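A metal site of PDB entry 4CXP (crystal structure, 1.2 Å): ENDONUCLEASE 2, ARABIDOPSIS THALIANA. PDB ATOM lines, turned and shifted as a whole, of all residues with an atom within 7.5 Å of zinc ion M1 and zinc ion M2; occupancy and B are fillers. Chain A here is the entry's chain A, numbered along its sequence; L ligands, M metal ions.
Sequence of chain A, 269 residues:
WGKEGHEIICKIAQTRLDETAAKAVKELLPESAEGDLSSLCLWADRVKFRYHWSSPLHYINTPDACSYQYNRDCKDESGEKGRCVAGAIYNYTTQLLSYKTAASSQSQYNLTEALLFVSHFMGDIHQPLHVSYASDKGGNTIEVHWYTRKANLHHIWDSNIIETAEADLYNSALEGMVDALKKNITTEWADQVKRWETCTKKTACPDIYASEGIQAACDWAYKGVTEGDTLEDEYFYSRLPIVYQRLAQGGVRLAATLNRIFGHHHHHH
Four residues have an atom within 4 Å of zinc ion M2: Asp 45, His 58, His 120 and Asp 124. Along chain A the residues within 4 Å of zinc ion M2 span positions 45 to 124.
Of the 25 residues printed, 4 come within 4 Å of zinc ion M1. The nearest printed residue that does not touch zinc ion M1 is Gly 2 (4.3 Å).
Zinc ion M2 is bound by the side-chain carboxylate (OD2) of Asp 124 (2.2 Å), an oxygen (O4) of the ligand (2.2 Å), a ring nitrogen (ND1) of His 58 (2.2 Å), a ring nitrogen (NE2) of His 120 (2.2 Å), an oxygen (O2) of the ligand (2.3 Å) and the side-chain carboxylate (OD1) of Asp 45 (2.4 Å). Zinc ion M2 has six donor atoms within binding distance.
Zinc ion M1 is bound by O4 of the ligand (1.9 Å), NE2 of His 6 (2.0 Å), OD1 of Asp 124 (2.1 Å), N of Trp 1 (2.1 Å) and O of Trp 1 (2.3 Å).
The indole nitrogen (NE1) of Trp 1 is in hydrogen-bond range of the backbone carbonyl oxygen (O) of Gly 123 (2.8 Å). A ring nitrogen (ND1) of His 130 sits at hydrogen-bond distance from the backbone carbonyl oxygen (O) of His 58, at 2.7 Å. ND1 of His 120 lies within hydrogen-bond range of O of Cys 41, at 2.8 Å. The side-chain amino group (NZ) of Lys 48 sits close to the side-chain carboxylate (OD1) of Asp 45 (3.3 Å).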
ATOM      1  N   TRP A   1      26.385   0.644  24.112  1.00  0.00           N
ATOM      2  CA  TRP A   1      25.768   0.989  22.812  1.00  0.00           C
ATOM      3  C   TRP A   1      26.842   1.082  21.756  1.00  0.00           C
ATOM      4  O   TRP A   1      28.005   1.342  22.072  1.00  0.00           O
ATOM      5  CB  TRP A   1      25.066   2.352  22.869  1.00  0.00           C
ATOM      6  CG  TRP A   1      24.057   2.518  23.980  1.00  0.00           C
ATOM      7  CD1 TRP A   1      24.279   3.120  25.164  1.00  0.00           C
ATOM      8  CD2 TRP A   1      22.688   2.093  23.996  1.00  0.00           C
ATOM      9  NE1 TRP A   1      23.143   3.111  25.922  1.00  0.00           N
ATOM     10  CE2 TRP A   1      22.144   2.486  25.224  1.00  0.00           C
ATOM     11  CE3 TRP A   1      21.870   1.412  23.090  1.00  0.00           C
ATOM     12  CZ2 TRP A   1      20.827   2.231  25.564  1.00  0.00           C
ATOM     13  CZ3 TRP A   1      20.551   1.154  23.440  1.00  0.00           C
ATOM     14  CH2 TRP A   1      20.047   1.567  24.661  1.00  0.00           C
ATOM     15  N   GLY A   2      26.427   0.970  20.504  1.00  0.00           N
ATOM     16  CA  GLY A   2      27.260   1.366  19.380  1.00  0.00           C
ATOM     17  C   GLY A   2      27.277   2.861  19.181  1.00  0.00           C
ATOM     18  O   GLY A   2      26.822   3.652  20.017  1.00  0.00           O
ATOM     19  N   LYS A   3      27.810   3.281  18.048  1.00  0.00           N
ATOM     20  CA  LYS A   3      28.059   4.670  17.787  1.00  0.00           C
ATOM     21  C   LYS A   3      26.810   5.512  17.894  1.00  0.00           C
ATOM     22  O   LYS A   3      26.826   6.599  18.474  1.00  0.00           O
ATOM     23  CB  LYS A   3      28.671   4.813  16.384  1.00  0.00           C
ATOM     24  CG  LYS A   3      28.843   6.229  15.890  1.00  0.00           C
ATOM     25  CD  LYS A   3      29.384   6.232  14.464  1.00  0.00           C
ATOM     26  CE  LYS A   3      29.708   7.627  13.956  1.00  0.00           C
ATOM     27  NZ  LYS A   3      28.522   8.267  13.309  1.00  0.00           N
ATOM     28  N   GLY A   5      23.896   5.102  19.463  1.00  0.00           N
ATOM     29  CA  GLY A   5      23.349   5.293  20.793  1.00  0.00           C
ATOM     30  C   GLY A   5      24.133   6.298  21.600  1.00  0.00           C
ATOM     31  O   GLY A   5      23.560   7.155  22.268  1.00  0.00           O
ATOM     32  N   HIS A   6      25.471   6.183  21.587  1.00  0.00           N
ATOM     33  CA  HIS A   6      26.286   7.155  22.318  1.00  0.00           C
ATOM     34  C   HIS A   6      26.139   8.563  21.760  1.00  0.00           C
ATOM     35  O   HIS A   6      26.125   9.534  22.513  1.00  0.00           O
ATOM     36  CB  HIS A   6      27.753   6.743  22.348  1.00  0.00           C
ATOM     37  CG  HIS A   6      27.985   5.581  23.238  1.00  0.00           C
ATOM     38  ND1 HIS A   6      27.944   5.673  24.614  1.00  0.00           N
ATOM     39  CD2 HIS A   6      28.160   4.268  22.958  1.00  0.00           C
ATOM     40  CE1 HIS A   6      28.104   4.457  25.122  1.00  0.00           C
ATOM     41  NE2 HIS A   6      28.235   3.585  24.146  1.00  0.00           N
ATOM     42  N   CYS A  41      32.165  10.481  21.934  1.00  0.00           N
ATOM     43  CA  CYS A  41      31.493   9.629  22.926  1.00  0.00           C
ATOM     44  C   CYS A  41      31.672   8.126  22.680  1.00  0.00           C
ATOM     45  O   CYS A  41      31.192   7.350  23.492  1.00  0.00           O
ATOM     46  CB  CYS A  41      30.014  10.030  23.156  1.00  0.00           C
ATOM     47  SG  CYS A  41      29.935  11.487  24.220  1.00  0.00           S
ATOM     48  N   LEU A  42      32.443   7.745  21.667  1.00  0.00           N
ATOM     49  CA  LEU A  42      32.925   6.366  21.481  1.00  0.00           C
ATOM     50  C   LEU A  42      34.409   6.203  21.786  1.00  0.00           C
ATOM     51  O   LEU A  42      34.943   5.093  21.697  1.00  0.00           O
ATOM     52  CB  LEU A  42      32.603   5.836  20.072  1.00  0.00           C
ATOM     53  CG  LEU A  42      32.044   4.415  19.955  1.00  0.00           C
ATOM     54  CD1 LEU A  42      30.746   4.210  20.686  1.00  0.00           C
ATOM     55  CD2 LEU A  42      31.889   4.070  18.486  1.00  0.00           C
ATOM     56  N   ALA A  44      35.977   5.919  24.509  1.00  0.00           N
ATOM     57  CA  ALA A  44      36.276   4.898  25.495  1.00  0.00           C
ATOM     58  C   ALA A  44      36.331   3.504  24.868  1.00  0.00           C
ATOM     59  O   ALA A  44      37.113   2.658  25.281  1.00  0.00           O
ATOM     60  CB  ALA A  44      35.282   4.932  26.638  1.00  0.00           C
ATOM     61  N   ASP A  45      35.458   3.241  23.906  1.00  0.00           N
ATOM     62  CA  ASP A  45      35.519   1.930  23.250  1.00  0.00           C
ATOM     63  C   ASP A  45      36.835   1.723  22.495  1.00  0.00           C
ATOM     64  O   ASP A  45      37.280   0.585  22.388  1.00  0.00           O
ATOM     65  CB  ASP A  45      34.347   1.743  22.282  1.00  0.00           C
ATOM     66  CG  ASP A  45      33.093   1.252  22.933  1.00  0.00           C
ATOM     67  OD1 ASP A  45      33.054   0.912  24.116  1.00  0.00           O
ATOM     68  OD2 ASP A  45      32.091   1.223  22.186  1.00  0.00           O
ATOM     69  N   ARG A  46      37.443   2.799  22.038  1.00  0.00           N
ATOM     70  CA  ARG A  46      38.676   2.746  21.253  1.00  0.00           C
ATOM     71  C   ARG A  46      39.944   2.652  22.102  1.00  0.00           C
ATOM     72  O   ARG A  46      41.026   2.599  21.548  1.00  0.00           O
ATOM     73  CB  ARG A  46      38.772   3.948  20.322  1.00  0.00           C
ATOM     74  CG  ARG A  46      37.732   3.924  19.228  1.00  0.00           C
ATOM     75  CD  ARG A  46      38.064   4.943  18.140  1.00  0.00           C
ATOM     76  NE  ARG A  46      37.992   6.314  18.630  1.00  0.00           N
ATOM     77  CZ  ARG A  46      39.036   7.077  18.931  1.00  0.00           C
ATOM     78  NH1 ARG A  46      40.289   6.632  18.786  1.00  0.00           N
ATOM     79  NH2 ARG A  46      38.820   8.305  19.358  1.00  0.00           N
ATOM     80  N   LYS A  48      39.859   0.222  24.768  1.00  0.00           N
ATOM     81  CA  LYS A  48      39.662  -1.056  25.453  1.00  0.00           C
ATOM     82  C   LYS A  48      40.892  -1.929  25.504  1.00  0.00           C
ATOM     83  O   LYS A  48      41.029  -2.726  26.430  1.00  0.00           O
ATOM     84  CB  LYS A  48      38.496  -1.854  24.829  1.00  0.00           C
ATOM     85  CG  LYS A  48      37.133  -1.371  25.256  1.00  0.00           C
ATOM     86  CD  LYS A  48      36.043  -2.137  24.520  1.00  0.00           C
ATOM     87  CE  LYS A  48      34.656  -1.699  24.961  1.00  0.00           C
ATOM     88  NZ  LYS A  48      33.608  -2.335  24.121  1.00  0.00           N
ATOM     89  N   SER A  55      38.558  -2.331  30.065  1.00  0.00           N
ATOM     90  CA  SER A  55      37.571  -3.135  29.363  1.00  0.00           C
ATOM     91  C   SER A  55      36.389  -3.547  30.264  1.00  0.00           C
ATOM     92  O   SER A  55      35.239  -3.409  29.859  1.00  0.00           O
ATOM     93  CB  SER A  55      38.232  -4.309  28.626  1.00  0.00           C
ATOM     94  OG  SER A  55      38.664  -3.935  27.320  1.00  0.00           O
ATOM     95  N   LEU A  57      35.136  -2.010  32.665  1.00  0.00           N
ATOM     96  CA  LEU A  57      34.431  -0.829  33.127  1.00  0.00           C
ATOM     97  C   LEU A  57      33.227  -0.459  32.275  1.00  0.00           C
ATOM     98  O   LEU A  57      32.513   0.474  32.624  1.00  0.00           O
ATOM     99  CB  LEU A  57      35.403   0.369  33.202  1.00  0.00           C
ATOM    100  CG  LEU A  57      36.638   0.160  34.075  1.00  0.00           C
ATOM    101  CD1 LEU A  57      37.453   1.446  34.095  1.00  0.00           C
ATOM    102  CD2 LEU A  57      36.323  -0.312  35.487  1.00  0.00           C
ATOM    103  N   HIS A  58      32.999  -1.176  31.175  1.00  0.00           N
ATOM    104  CA  HIS A  58      31.862  -0.867  30.299  1.00  0.00           C
ATOM    105  C   HIS A  58      30.571  -1.551  30.719  1.00  0.00           C
ATOM    106  O   HIS A  58      29.516  -1.215  30.188  1.00  0.00           O
ATOM    107  CB  HIS A  58      32.172  -1.239  28.854  1.00  0.00           C
ATOM    108  CG  HIS A  58      33.252  -0.395  28.261  1.00  0.00           C
ATOM    109  ND1 HIS A  58      33.032   0.477  27.220  1.00  0.00           N
ATOM    110  CD2 HIS A  58      34.552  -0.274  28.613  1.00  0.00           C
ATOM    111  CE1 HIS A  58      34.174   1.107  26.964  1.00  0.00           C
ATOM    112  NE2 HIS A  58      35.114   0.666  27.790  1.00  0.00           N
ATOM    113  N   TYR A  59      30.621  -2.504  31.656  1.00  0.00           N
ATOM    114  CA  TYR A  59      29.442  -3.316  31.938  1.00  0.00           C
ATOM    115  C   TYR A  59      29.437  -3.770  33.384  1.00  0.00           C
ATOM    116  O   TYR A  59      30.360  -3.501  34.158  1.00  0.00           O
ATOM    117  CB  TYR A  59      29.381  -4.507  30.937  1.00  0.00           C
ATOM    118  CG  TYR A  59      30.610  -5.369  31.001  1.00  0.00           C
ATOM    119  CD1 TYR A  59      30.761  -6.364  31.982  1.00  0.00           C
ATOM    120  CD2 TYR A  59      31.664  -5.170  30.118  1.00  0.00           C
ATOM    121  CE1 TYR A  59      31.906  -7.125  32.044  1.00  0.00           C
ATOM    122  CE2 TYR A  59      32.812  -5.932  30.201  1.00  0.00           C
ATOM    123  CZ  TYR A  59      32.934  -6.908  31.160  1.00  0.00           C
ATOM    124  OH  TYR A  59      34.088  -7.651  31.229  1.00  0.00           O
ATOM    125  N   VAL A  85      30.959  -0.775  35.377  1.00  0.00           N
ATOM    126  CA  VAL A  85      30.552   0.542  34.882  1.00  0.00           C
ATOM    127  C   VAL A  85      30.055   1.461  36.000  1.00  0.00           C
ATOM    128  O   VAL A  85      30.263   2.674  35.915  1.00  0.00           O
ATOM    129  CB  VAL A  85      29.567   0.406  33.696  1.00  0.00           C
ATOM    130  CG1 VAL A  85      28.226  -0.175  34.090  1.00  0.00           C
ATOM    131  CG2 VAL A  85      29.419   1.705  32.958  1.00  0.00           C
ATOM    132  N   HIS A 120      30.745   8.291  28.090  1.00  0.00           N
ATOM    133  CA  HIS A 120      30.513   6.977  27.515  1.00  0.00           C
ATOM    134  C   HIS A 120      29.866   6.029  28.518  1.00  0.00           C
ATOM    135  O   HIS A 120      28.910   5.323  28.190  1.00  0.00           O
ATOM    136  CB  HIS A 120      31.845   6.388  27.030  1.00  0.00           C
ATOM    137  CG  HIS A 120      31.685   5.091  26.317  1.00  0.00           C
ATOM    138  ND1 HIS A 120      31.490   5.006  24.963  1.00  0.00           N
ATOM    139  CD2 HIS A 120      31.720   3.811  26.768  1.00  0.00           C
ATOM    140  CE1 HIS A 120      31.377   3.733  24.618  1.00  0.00           C
ATOM    141  NE2 HIS A 120      31.534   2.986  25.690  1.00  0.00           N
ATOM    142  N   PHE A 121      30.398   5.982  29.732  1.00  0.00           N
ATOM    143  CA  PHE A 121      29.899   5.033  30.726  1.00  0.00           C
ATOM    144  C   PHE A 121      28.487   5.372  31.209  1.00  0.00           C
ATOM    145  O   PHE A 121      27.710   4.465  31.471  1.00  0.00           O
ATOM    146  CB  PHE A 121      30.886   4.921  31.898  1.00  0.00           C
ATOM    147  CG  PHE A 121      32.208   4.301  31.519  1.00  0.00           C
ATOM    148  CD1 PHE A 121      32.300   3.295  30.582  1.00  0.00           C
ATOM    149  CD2 PHE A 121      33.373   4.719  32.145  1.00  0.00           C
ATOM    150  CE1 PHE A 121      33.528   2.736  30.262  1.00  0.00           C
ATOM    151  CE2 PHE A 121      34.595   4.168  31.825  1.00  0.00           C
ATOM    152  CZ  PHE A 121      34.669   3.175  30.878  1.00  0.00           C
ATOM    153  N   GLY A 123      26.299   6.430  29.248  1.00  0.00           N
ATOM    154  CA  GLY A 123      25.567   5.752  28.225  1.00  0.00           C
ATOM    155  C   GLY A 123      25.497   4.256  28.401  1.00  0.00           C
ATOM    156  O   GLY A 123      24.410   3.659  28.381  1.00  0.00           O
ATOM    157  N   ASP A 124      26.638   3.605  28.588  1.00  0.00           N
ATOM    158  CA  ASP A 124      26.663   2.152  28.682  1.00  0.00           C
ATOM    159  C   ASP A 124      25.818   1.631  29.832  1.00  0.00           C
ATOM    160  O   ASP A 124      25.184   0.596  29.698  1.00  0.00           O
ATOM    161  CB  ASP A 124      28.097   1.622  28.746  1.00  0.00           C
ATOM    162  CG  ASP A 124      28.726   1.371  27.386  1.00  0.00           C
ATOM    163  OD1 ASP A 124      28.027   1.597  26.386  1.00  0.00           O
ATOM    164  OD2 ASP A 124      29.887   0.956  27.377  1.00  0.00           O
ATOM    165  N   ILE A 125      25.796   2.315  30.993  1.00  0.00           N
ATOM    166  CA  ILE A 125      25.025   1.826  32.126  1.00  0.00           C
ATOM    167  C   ILE A 125      23.536   1.869  31.851  1.00  0.00           C
ATOM    168  O   ILE A 125      22.769   1.273  32.606  1.00  0.00           O
ATOM    169  CB  ILE A 125      25.405   2.537  33.429  1.00  0.00           C
ATOM    170  CG1 ILE A 125      25.032   1.700  34.643  1.00  0.00           C
ATOM    171  CG2 ILE A 125      24.805   3.940  33.488  1.00  0.00           C
ATOM    172  CD1 ILE A 125      25.652   2.217  35.925  1.00  0.00           C
ATOM    173  N   GLN A 127      22.328   0.828  28.738  1.00  0.00           N
ATOM    174  CA  GLN A 127      22.030  -0.246  27.790  1.00  0.00           C
ATOM    175  C   GLN A 127      21.654  -1.463  28.642  1.00  0.00           C
ATOM    176  O   GLN A 127      22.472  -1.931  29.433  1.00  0.00           O
ATOM    177  CB  GLN A 127      23.272  -0.498  26.920  1.00  0.00           C
ATOM    178  CG  GLN A 127      23.025  -1.047  25.522  1.00  0.00           C
ATOM    179  CD  GLN A 127      22.644  -2.516  25.465  1.00  0.00           C
ATOM    180  OE1 GLN A 127      21.646  -2.920  26.071  1.00  0.00           O
ATOM    181  NE2 GLN A 127      23.400  -3.314  24.727  1.00  0.00           N
ATOM    182  N   HIS A 130      24.119  -4.234  29.077  1.00  0.00           N
ATOM    183  CA  HIS A 130      25.358  -3.921  29.798  1.00  0.00           C
ATOM    184  C   HIS A 130      25.238  -4.141  31.303  1.00  0.00           C
ATOM    185  O   HIS A 130      26.218  -3.970  31.988  1.00  0.00           O
ATOM    186  CB  HIS A 130      25.825  -2.500  29.489  1.00  0.00           C
ATOM    187  CG  HIS A 130      26.583  -2.409  28.200  1.00  0.00           C
ATOM    188  ND1 HIS A 130      27.875  -1.986  28.124  1.00  0.00           N
ATOM    189  CD2 HIS A 130      26.239  -2.755  26.932  1.00  0.00           C
ATOM    190  CE1 HIS A 130      28.302  -2.077  26.879  1.00  0.00           C
ATOM    191  NE2 HIS A 130      27.317  -2.547  26.131  1.00  0.00           N
ATOM    192  N   HIS A 154      23.134  -9.137  22.251  1.00  0.00           N
ATOM    193  CA  HIS A 154      23.798  -7.950  22.730  1.00  0.00           C
ATOM    194  C   HIS A 154      23.929  -6.881  21.632  1.00  0.00           C
ATOM    195  O   HIS A 154      23.633  -5.704  21.847  1.00  0.00           O
ATOM    196  CB  HIS A 154      25.166  -8.296  23.340  1.00  0.00           C
ATOM    197  CG  HIS A 154      25.804  -7.121  23.991  1.00  0.00           C
ATOM    198  ND1 HIS A 154      25.758  -6.916  25.344  1.00  0.00           N
ATOM    199  CD2 HIS A 154      26.423  -6.042  23.474  1.00  0.00           C
ATOM    200  CE1 HIS A 154      26.353  -5.776  25.635  1.00  0.00           C
ATOM    201  NE2 HIS A 154      26.752  -5.205  24.503  1.00  0.00           N
ATOM    202  N   ASP A 158      22.866  -3.039  21.271  1.00  0.00           N
ATOM    203  CA  ASP A 158      23.843  -1.973  21.066  1.00  0.00           C
ATOM    204  C   ASP A 158      23.535  -1.169  19.795  1.00  0.00           C
ATOM    205  O   ASP A 158      23.722   0.056  19.804  1.00  0.00           O
ATOM    206  CB  ASP A 158      25.263  -2.527  20.898  1.00  0.00           C
ATOM    207  CG  ASP A 158      26.027  -2.746  22.191  1.00  0.00           C
ATOM    208  OD1 ASP A 158      25.626  -2.267  23.273  1.00  0.00           O
ATOM    209  OD2 ASP A 158      27.111  -3.388  22.102  1.00  0.00           O
HETATM  210  S1  LIG L   1      30.132  -0.873  23.922  1.00  0.00           S
HETATM  211  O1  LIG L   1      30.837  -0.931  22.580  1.00  0.00           O
HETATM  212  O2  LIG L   1      31.096  -1.404  25.058  1.00  0.00           O
HETATM  213  O3  LIG L   1      28.796  -1.552  23.706  1.00  0.00           O
HETATM  214  O4  LIG L   1      29.923   0.573  24.242  1.00  0.00           O
HETATM  215 ZN    ZN M   1      28.256   1.580  24.320  1.00  0.00          ZN
HETATM  216 ZN    ZN M   2      31.377   0.799  25.826  1.00  0.00          ZN
HETATM  217 ZN    ZN M   3      27.710  -3.296  24.176  1.00  0.00          ZN
